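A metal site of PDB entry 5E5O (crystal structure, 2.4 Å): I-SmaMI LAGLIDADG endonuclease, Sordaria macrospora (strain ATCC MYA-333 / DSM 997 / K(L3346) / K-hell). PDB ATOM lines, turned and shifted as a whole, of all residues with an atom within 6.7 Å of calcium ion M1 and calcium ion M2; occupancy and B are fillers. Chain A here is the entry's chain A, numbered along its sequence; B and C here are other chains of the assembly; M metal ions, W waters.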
ATOM      1  N   ASP A  18      10.611  29.143 -37.590  1.00  0.00           N
ATOM      2  CA  ASP A  18      11.134  28.047 -36.798  1.00  0.00           C
ATOM      3  C   ASP A  18      10.328  27.854 -35.528  1.00  0.00           C
ATOM      4  O   ASP A  18      10.018  26.720 -35.154  1.00  0.00           O
ATOM      5  CB  ASP A  18      12.636  28.242 -36.448  1.00  0.00           C
ATOM      6  CG  ASP A  18      13.550  27.395 -37.293  1.00  0.00           C
ATOM      7  OD1 ASP A  18      13.227  26.204 -37.526  1.00  0.00           O
ATOM      8  OD2 ASP A  18      14.631  27.874 -37.644  1.00  0.00           O
ATOM      9  N   ALA A  19       9.932  28.952 -34.897  1.00  0.00           N
ATOM     10  CA  ALA A  19       9.156  28.931 -33.676  1.00  0.00           C
ATOM     11  C   ALA A  19       7.684  28.774 -33.912  1.00  0.00           C
ATOM     12  O   ALA A  19       7.075  28.090 -33.118  1.00  0.00           O
ATOM     13  CB  ALA A  19       9.407  30.220 -32.855  1.00  0.00           C
ATOM     14  N   GLU A  20       7.064  29.491 -34.872  1.00  0.00           N
ATOM     15  CA  GLU A  20       5.558  29.523 -34.990  1.00  0.00           C
ATOM     16  C   GLU A  20       4.893  28.999 -36.305  1.00  0.00           C
ATOM     17  O   GLU A  20       3.698  28.659 -36.338  1.00  0.00           O
ATOM     18  CB  GLU A  20       4.961  30.924 -34.711  1.00  0.00           C
ATOM     19  CG  GLU A  20       5.105  31.598 -33.351  1.00  0.00           C
ATOM     20  CD  GLU A  20       4.485  30.839 -32.186  1.00  0.00           C
ATOM     21  OE1 GLU A  20       3.255  30.937 -31.945  1.00  0.00           O
ATOM     22  OE2 GLU A  20       5.238  30.155 -31.436  1.00  0.00           O
ATOM     23  N   GLY A  21       5.577  28.875 -37.392  1.00  0.00           N
ATOM     24  CA  GLY A  21       4.900  28.260 -38.580  1.00  0.00           C
ATOM     25  C   GLY A  21       4.425  26.819 -38.517  1.00  0.00           C
ATOM     26  O   GLY A  21       4.874  26.030 -37.689  1.00  0.00           O
ATOM     27  N   LYS A 103      11.426  21.646 -37.237  1.00  0.00           N
ATOM     28  CA  LYS A 103      10.521  22.143 -38.249  1.00  0.00           C
ATOM     29  C   LYS A 103      11.172  22.016 -39.659  1.00  0.00           C
ATOM     30  O   LYS A 103      10.476  21.946 -40.651  1.00  0.00           O
ATOM     31  CB  LYS A 103      10.246  23.613 -37.943  1.00  0.00           C
ATOM     32  CG  LYS A 103       9.142  24.332 -38.720  1.00  0.00           C
ATOM     33  CD  LYS A 103       7.801  24.258 -38.039  1.00  0.00           C
ATOM     34  CE  LYS A 103       7.800  24.913 -36.682  1.00  0.00           C
ATOM     35  NZ  LYS A 103       6.994  26.171 -36.548  1.00  0.00           N
ATOM     36  N   PHE A 175      13.154  34.086 -33.379  1.00  0.00           N
ATOM     37  CA  PHE A 175      12.678  32.885 -32.728  1.00  0.00           C
ATOM     38  C   PHE A 175      12.072  33.192 -31.362  1.00  0.00           C
ATOM     39  O   PHE A 175      11.083  32.623 -30.986  1.00  0.00           O
ATOM     40  CB  PHE A 175      13.818  31.900 -32.644  1.00  0.00           C
ATOM     41  CG  PHE A 175      13.470  30.642 -31.994  1.00  0.00           C
ATOM     42  CD1 PHE A 175      12.776  29.709 -32.680  1.00  0.00           C
ATOM     43  CD2 PHE A 175      13.999  30.324 -30.766  1.00  0.00           C
ATOM     44  CE1 PHE A 175      12.459  28.501 -32.127  1.00  0.00           C
ATOM     45  CE2 PHE A 175      13.766  29.104 -30.205  1.00  0.00           C
ATOM     46  CZ  PHE A 175      12.956  28.201 -30.904  1.00  0.00           C
ATOM     47  N   SER A 177      10.720  35.912 -30.503  1.00  0.00           N
ATOM     48  CA  SER A 177       9.443  36.553 -30.729  1.00  0.00           C
ATOM     49  C   SER A 177       8.309  35.566 -30.736  1.00  0.00           C
ATOM     50  O   SER A 177       7.261  35.898 -30.243  1.00  0.00           O
ATOM     51  CB  SER A 177       9.464  37.415 -32.001  1.00  0.00           C
ATOM     52  OG  SER A 177      10.560  38.327 -31.935  1.00  0.00           O
ATOM     53  N   GLY A 178       8.518  34.344 -31.255  1.00  0.00           N
ATOM     54  CA  GLY A 178       7.454  33.325 -31.300  1.00  0.00           C
ATOM     55  C   GLY A 178       7.328  32.464 -30.053  1.00  0.00           C
ATOM     56  O   GLY A 178       6.262  32.279 -29.488  1.00  0.00           O
ATOM     57  N   ASP A 179       8.437  31.916 -29.655  1.00  0.00           N
ATOM     58  CA  ASP A 179       8.547  31.182 -28.429  1.00  0.00           C
ATOM     59  C   ASP A 179       9.539  31.948 -27.592  1.00  0.00           C
ATOM     60  O   ASP A 179      10.510  32.394 -28.117  1.00  0.00           O
ATOM     61  CB  ASP A 179       9.066  29.815 -28.735  1.00  0.00           C
ATOM     62  CG  ASP A 179       8.118  29.000 -29.510  1.00  0.00           C
ATOM     63  OD1 ASP A 179       6.937  29.285 -29.413  1.00  0.00           O
ATOM     64  OD2 ASP A 179       8.475  28.030 -30.202  1.00  0.00           O
ATOM     65  N   GLY A 180       9.305  32.140 -26.310  1.00  0.00           N
ATOM     66  CA  GLY A 180      10.174  33.031 -25.493  1.00  0.00           C
ATOM     67  C   GLY A 180       9.317  33.838 -24.562  1.00  0.00           C
ATOM     68  O   GLY A 180       8.331  34.348 -25.016  1.00  0.00           O
ATOM     69  N   THR A 205      10.849  27.943 -24.087  1.00  0.00           N
ATOM     70  CA  THR A 205      10.268  26.591 -24.126  1.00  0.00           C
ATOM     71  C   THR A 205      10.324  25.988 -25.527  1.00  0.00           C
ATOM     72  O   THR A 205      10.108  26.676 -26.544  1.00  0.00           O
ATOM     73  CB  THR A 205       8.819  26.596 -23.552  1.00  0.00           C
ATOM     74  OG1 THR A 205       8.777  27.331 -22.314  1.00  0.00           O
ATOM     75  CG2 THR A 205       8.303  25.181 -23.321  1.00  0.00           C
ATOM     76  N   GLN A 206      10.646  24.706 -25.597  1.00  0.00           N
ATOM     77  CA  GLN A 206      10.660  23.920 -26.842  1.00  0.00           C
ATOM     78  C   GLN A 206      10.468  22.488 -26.507  1.00  0.00           C
ATOM     79  O   GLN A 206      10.966  22.044 -25.505  1.00  0.00           O
ATOM     80  CB  GLN A 206      12.008  23.878 -27.542  1.00  0.00           C
ATOM     81  CG  GLN A 206      12.304  24.927 -28.555  1.00  0.00           C
ATOM     82  CD  GLN A 206      11.156  25.305 -29.536  1.00  0.00           C
ATOM     83  OE1 GLN A 206      10.349  26.241 -29.208  1.00  0.00           O
ATOM     84  NE2 GLN A 206      11.134  24.652 -30.726  1.00  0.00           N
ATOM     85  N   LYS A 262       4.931  41.417 -27.981  1.00  0.00           N
ATOM     86  CA  LYS A 262       5.979  40.973 -27.029  1.00  0.00           C
ATOM     87  C   LYS A 262       7.122  41.962 -26.881  1.00  0.00           C
ATOM     88  O   LYS A 262       7.738  41.972 -25.829  1.00  0.00           O
ATOM     89  CB  LYS A 262       6.562  39.650 -27.406  1.00  0.00           C
ATOM     90  CG  LYS A 262       7.400  39.069 -26.271  1.00  0.00           C
ATOM     91  CD  LYS A 262       7.857  37.672 -26.573  1.00  0.00           C
ATOM     92  CE  LYS A 262       6.705  36.703 -26.380  1.00  0.00           C
ATOM     93  NZ  LYS A 262       6.998  35.587 -27.298  1.00  0.00           N
ATOM     94  P    DA B  14       2.883  18.496 -27.742  1.00  0.00           P
ATOM     95  OP1  DA B  14       2.412  17.549 -28.818  1.00  0.00           O
ATOM     96  OP2  DA B  14       4.183  18.252 -27.158  1.00  0.00           O
ATOM     97  O5'  DA B  14       2.619  19.965 -28.276  1.00  0.00           O
ATOM     98  C5'  DA B  14       3.437  20.692 -29.164  1.00  0.00           C
ATOM     99  C4'  DA B  14       3.478  22.128 -28.683  1.00  0.00           C
ATOM    100  O4'  DA B  14       2.514  22.439 -27.620  1.00  0.00           O
ATOM    101  C3'  DA B  14       4.835  22.554 -28.123  1.00  0.00           C
ATOM    102  O3'  DA B  14       5.015  23.863 -28.671  1.00  0.00           O
ATOM    103  C2'  DA B  14       4.628  22.448 -26.613  1.00  0.00           C
ATOM    104  C1'  DA B  14       3.221  22.971 -26.494  1.00  0.00           C
ATOM    105  N9   DA B  14       2.457  22.621 -25.300  1.00  0.00           N
ATOM    106  C8   DA B  14       2.502  21.461 -24.561  1.00  0.00           C
ATOM    107  N7   DA B  14       1.569  21.392 -23.645  1.00  0.00           N
ATOM    108  C5   DA B  14       0.882  22.591 -23.779  1.00  0.00           C
ATOM    109  C6   DA B  14      -0.220  23.135 -23.079  1.00  0.00           C
ATOM    110  N6   DA B  14      -0.840  22.511 -22.077  1.00  0.00           N
ATOM    111  N1   DA B  14      -0.680  24.334 -23.482  1.00  0.00           N
ATOM    112  C2   DA B  14      -0.088  24.942 -24.513  1.00  0.00           C
ATOM    113  N3   DA B  14       0.958  24.542 -25.237  1.00  0.00           N
ATOM    114  C4   DA B  14       1.401  23.341 -24.806  1.00  0.00           C
ATOM    115  P    DT B  15       6.434  24.417 -28.987  1.00  0.00           P
ATOM    116  OP1  DT B  15       6.310  25.637 -29.781  1.00  0.00           O
ATOM    117  OP2  DT B  15       7.356  23.329 -29.392  1.00  0.00           O
ATOM    118  O5'  DT B  15       7.115  24.628 -27.559  1.00  0.00           O
ATOM    119  C5'  DT B  15       6.861  25.542 -26.466  1.00  0.00           C
ATOM    120  C4'  DT B  15       5.584  26.334 -26.466  1.00  0.00           C
ATOM    121  O4'  DT B  15       4.679  25.564 -25.631  1.00  0.00           O
ATOM    122  C3'  DT B  15       5.743  27.689 -25.771  1.00  0.00           C
ATOM    123  O3'  DT B  15       5.161  28.809 -26.366  1.00  0.00           O
ATOM    124  C2'  DT B  15       5.069  27.513 -24.429  1.00  0.00           C
ATOM    125  C1'  DT B  15       4.065  26.413 -24.692  1.00  0.00           C
ATOM    126  N1   DT B  15       3.724  25.602 -23.521  1.00  0.00           N
ATOM    127  C2   DT B  15       2.658  26.039 -22.757  1.00  0.00           C
ATOM    128  O2   DT B  15       2.017  27.038 -23.014  1.00  0.00           O
ATOM    129  N3   DT B  15       2.362  25.231 -21.682  1.00  0.00           N
ATOM    130  C4   DT B  15       3.033  24.089 -21.294  1.00  0.00           C
ATOM    131  O4   DT B  15       2.660  23.473 -20.308  1.00  0.00           O
ATOM    132  C5   DT B  15       4.164  23.713 -22.119  1.00  0.00           C
ATOM    133  C7   DT B  15       4.942  22.482 -21.774  1.00  0.00           C
ATOM    134  C6   DT B  15       4.445  24.480 -23.178  1.00  0.00           C
ATOM    135  P    DC B  16       5.634  30.321 -25.930  1.00  0.00           P
ATOM    136  OP1  DC B  16       5.195  31.227 -27.058  1.00  0.00           O
ATOM    137  OP2  DC B  16       7.032  30.302 -25.420  1.00  0.00           O
ATOM    138  O5'  DC B  16       4.812  30.680 -24.623  1.00  0.00           O
ATOM    139  C5'  DC B  16       3.493  31.208 -24.737  1.00  0.00           C
ATOM    140  C4'  DC B  16       3.016  31.566 -23.362  1.00  0.00           C
ATOM    141  O4'  DC B  16       2.978  30.346 -22.604  1.00  0.00           O
ATOM    142  C3'  DC B  16       3.986  32.506 -22.631  1.00  0.00           C
ATOM    143  O3'  DC B  16       3.182  33.623 -22.279  1.00  0.00           O
ATOM    144  C2'  DC B  16       4.577  31.650 -21.515  1.00  0.00           C
ATOM    145  C1'  DC B  16       3.492  30.601 -21.312  1.00  0.00           C
ATOM    146  N1   DC B  16       3.873  29.324 -20.730  1.00  0.00           N
ATOM    147  C2   DC B  16       2.992  28.700 -19.854  1.00  0.00           C
ATOM    148  O2   DC B  16       1.941  29.276 -19.556  1.00  0.00           O
ATOM    149  N3   DC B  16       3.309  27.499 -19.316  1.00  0.00           N
ATOM    150  C4   DC B  16       4.449  26.902 -19.674  1.00  0.00           C
ATOM    151  N4   DC B  16       4.730  25.722 -19.106  1.00  0.00           N
ATOM    152  C5   DC B  16       5.358  27.491 -20.596  1.00  0.00           C
ATOM    153  C6   DC B  16       5.016  28.685 -21.117  1.00  0.00           C
ATOM    154  P    DA C  13      -5.336  32.762 -24.931  1.00  0.00           P
ATOM    155  OP1  DA C  13      -5.015  33.771 -23.921  1.00  0.00           O
ATOM    156  OP2  DA C  13      -6.662  32.696 -25.570  1.00  0.00           O
ATOM    157  O5'  DA C  13      -4.102  32.965 -25.934  1.00  0.00           O
ATOM    158  C5'  DA C  13      -2.719  33.129 -25.443  1.00  0.00           C
ATOM    159  C4'  DA C  13      -1.709  32.420 -26.328  1.00  0.00           C
ATOM    160  O4'  DA C  13      -1.950  30.992 -26.371  1.00  0.00           O
ATOM    161  C3'  DA C  13      -1.708  32.820 -27.800  1.00  0.00           C
ATOM    162  O3'  DA C  13      -0.512  32.254 -28.391  1.00  0.00           O
ATOM    163  C2'  DA C  13      -2.849  31.978 -28.323  1.00  0.00           C
ATOM    164  C1'  DA C  13      -2.470  30.653 -27.653  1.00  0.00           C
ATOM    165  N9   DA C  13      -3.554  29.753 -27.388  1.00  0.00           N
ATOM    166  C8   DA C  13      -4.868  30.028 -27.124  1.00  0.00           C
ATOM    167  N7   DA C  13      -5.549  28.997 -26.688  1.00  0.00           N
ATOM    168  C5   DA C  13      -4.599  27.982 -26.620  1.00  0.00           C
ATOM    169  C6   DA C  13      -4.690  26.636 -26.230  1.00  0.00           C
ATOM    170  N6   DA C  13      -5.826  26.058 -25.836  1.00  0.00           N
ATOM    171  N1   DA C  13      -3.552  25.907 -26.261  1.00  0.00           N
ATOM    172  C2   DA C  13      -2.421  26.487 -26.680  1.00  0.00           C
ATOM    173  N3   DA C  13      -2.215  27.731 -27.071  1.00  0.00           N
ATOM    174  C4   DA C  13      -3.359  28.449 -26.998  1.00  0.00           C
ATOM    175  P    DA C  14       0.335  33.095 -29.408  1.00  0.00           P
ATOM    176  OP1  DA C  14       1.548  33.566 -28.697  1.00  0.00           O
ATOM    177  OP2  DA C  14      -0.596  33.947 -30.206  1.00  0.00           O
ATOM    178  O5'  DA C  14       0.907  32.088 -30.511  1.00  0.00           O
ATOM    179  C5'  DA C  14       0.170  31.033 -31.092  1.00  0.00           C
ATOM    180  C4'  DA C  14       0.874  29.743 -30.751  1.00  0.00           C
ATOM    181  O4'  DA C  14      -0.069  28.907 -29.998  1.00  0.00           O
ATOM    182  C3'  DA C  14       1.228  28.930 -31.984  1.00  0.00           C
ATOM    183  O3'  DA C  14       2.380  28.103 -31.709  1.00  0.00           O
ATOM    184  C2'  DA C  14      -0.072  28.205 -32.255  1.00  0.00           C
ATOM    185  C1'  DA C  14      -0.503  27.828 -30.838  1.00  0.00           C
ATOM    186  N9   DA C  14      -1.942  27.646 -30.636  1.00  0.00           N
ATOM    187  C8   DA C  14      -2.945  28.559 -30.840  1.00  0.00           C
ATOM    188  N7   DA C  14      -4.125  28.123 -30.508  1.00  0.00           N
ATOM    189  C5   DA C  14      -3.891  26.837 -30.054  1.00  0.00           C
ATOM    190  C6   DA C  14      -4.752  25.844 -29.572  1.00  0.00           C
ATOM    191  N6   DA C  14      -6.067  26.001 -29.468  1.00  0.00           N
ATOM    192  N1   DA C  14      -4.201  24.672 -29.171  1.00  0.00           N
ATOM    193  C2   DA C  14      -2.878  24.528 -29.258  1.00  0.00           C
ATOM    194  N3   DA C  14      -1.962  25.398 -29.690  1.00  0.00           N
ATOM    195  C4   DA C  14      -2.552  26.536 -30.107  1.00  0.00           C
ATOM    196  P    DT C  15       2.966  27.107 -32.876  1.00  0.00           P
ATOM    197  OP1  DT C  15       4.366  26.858 -32.511  1.00  0.00           O
ATOM    198  OP2  DT C  15       2.591  27.609 -34.239  1.00  0.00           O
ATOM    199  O5'  DT C  15       2.054  25.802 -32.778  1.00  0.00           O
ATOM    200  C5'  DT C  15       2.291  24.931 -31.659  1.00  0.00           C
ATOM    201  C4'  DT C  15       1.841  23.529 -31.944  1.00  0.00           C
ATOM    202  O4'  DT C  15       0.395  23.438 -31.824  1.00  0.00           O
ATOM    203  C3'  DT C  15       2.180  22.999 -33.337  1.00  0.00           C
ATOM    204  O3'  DT C  15       2.458  21.608 -33.116  1.00  0.00           O
ATOM    205  C2'  DT C  15       0.931  23.352 -34.130  1.00  0.00           C
ATOM    206  C1'  DT C  15      -0.177  23.151 -33.088  1.00  0.00           C
ATOM    207  N1   DT C  15      -1.417  23.934 -33.183  1.00  0.00           N
ATOM    208  C2   DT C  15      -2.531  23.369 -32.624  1.00  0.00           C
ATOM    209  O2   DT C  15      -2.534  22.249 -32.140  1.00  0.00           O
ATOM    210  N3   DT C  15      -3.681  24.125 -32.726  1.00  0.00           N
ATOM    211  C4   DT C  15      -3.800  25.383 -33.297  1.00  0.00           C
ATOM    212  O4   DT C  15      -4.904  25.935 -33.304  1.00  0.00           O
ATOM    213  C5   DT C  15      -2.562  25.941 -33.821  1.00  0.00           C
ATOM    214  C7   DT C  15      -2.582  27.288 -34.465  1.00  0.00           C
ATOM    215  C6   DT C  15      -1.444  25.202 -33.724  1.00  0.00           C
HETATM  216 CA    CA M   1       4.770  30.458 -29.141  1.00  0.00          CA
HETATM  217 CA    CA M   2       6.163  27.412 -31.127  1.00  0.00          CA
HETATM  218  O   HOH W   1       7.282  25.717 -32.109  1.00  0.00           O
HETATM  219  O   HOH W   2       3.692  32.378 -29.190  1.00  0.00           O
HETATM  220  O   HOH W   3       3.848  28.032 -30.025  1.00  0.00           O
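OP2 of DC 16 of chain B lies within hydrogen-bond range of N of Gly 180.
OP2 of DT 15 of chain C sits close to the backbone carbonyl oxygen (O) of Glu 20.
OE1 of Gln 206 sits close to OD2 of Asp 179, 2.8 Å away.
Along chain A the residues within 4 Å of calcium ion M1 span positions 20 to 179.
The nearest printed residue that does not touch calcium ion M1 is DA 14 of chain C (4.2 Å).
DA 14 of chain C touches calcium ion M2.
Calcium ion M1 is bound by water W2 (2.2 Å), OP1 of DC 16 of chain B (2.3 Å), OE2 of Glu 20 (2.4 Å), O of Gly 178 (2.4 Å), OD1 of Asp 179 (2.5 Å) and water W3 (2.7 Å).
Calcium ion M2 is bound by OP1 of DT 15 of chain B (2.2 Å), water W1 (2.3 Å), O of Ala 19 (2.3 Å), OP1 of DT 15 of chain C (2.3 Å), OD2 of Asp 179 (2.6 Å), water W3 (2.6 Å) and OD1 of Asp 179 (2.7 Å).
Slightly farther from calcium ion M2 lies OE2 of Glu 20 (2.9 Å).
Water W2 lies within hydrogen-bond range of OP1 of DA 14 of chain C and the side-chain carboxylate of Glu 20.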
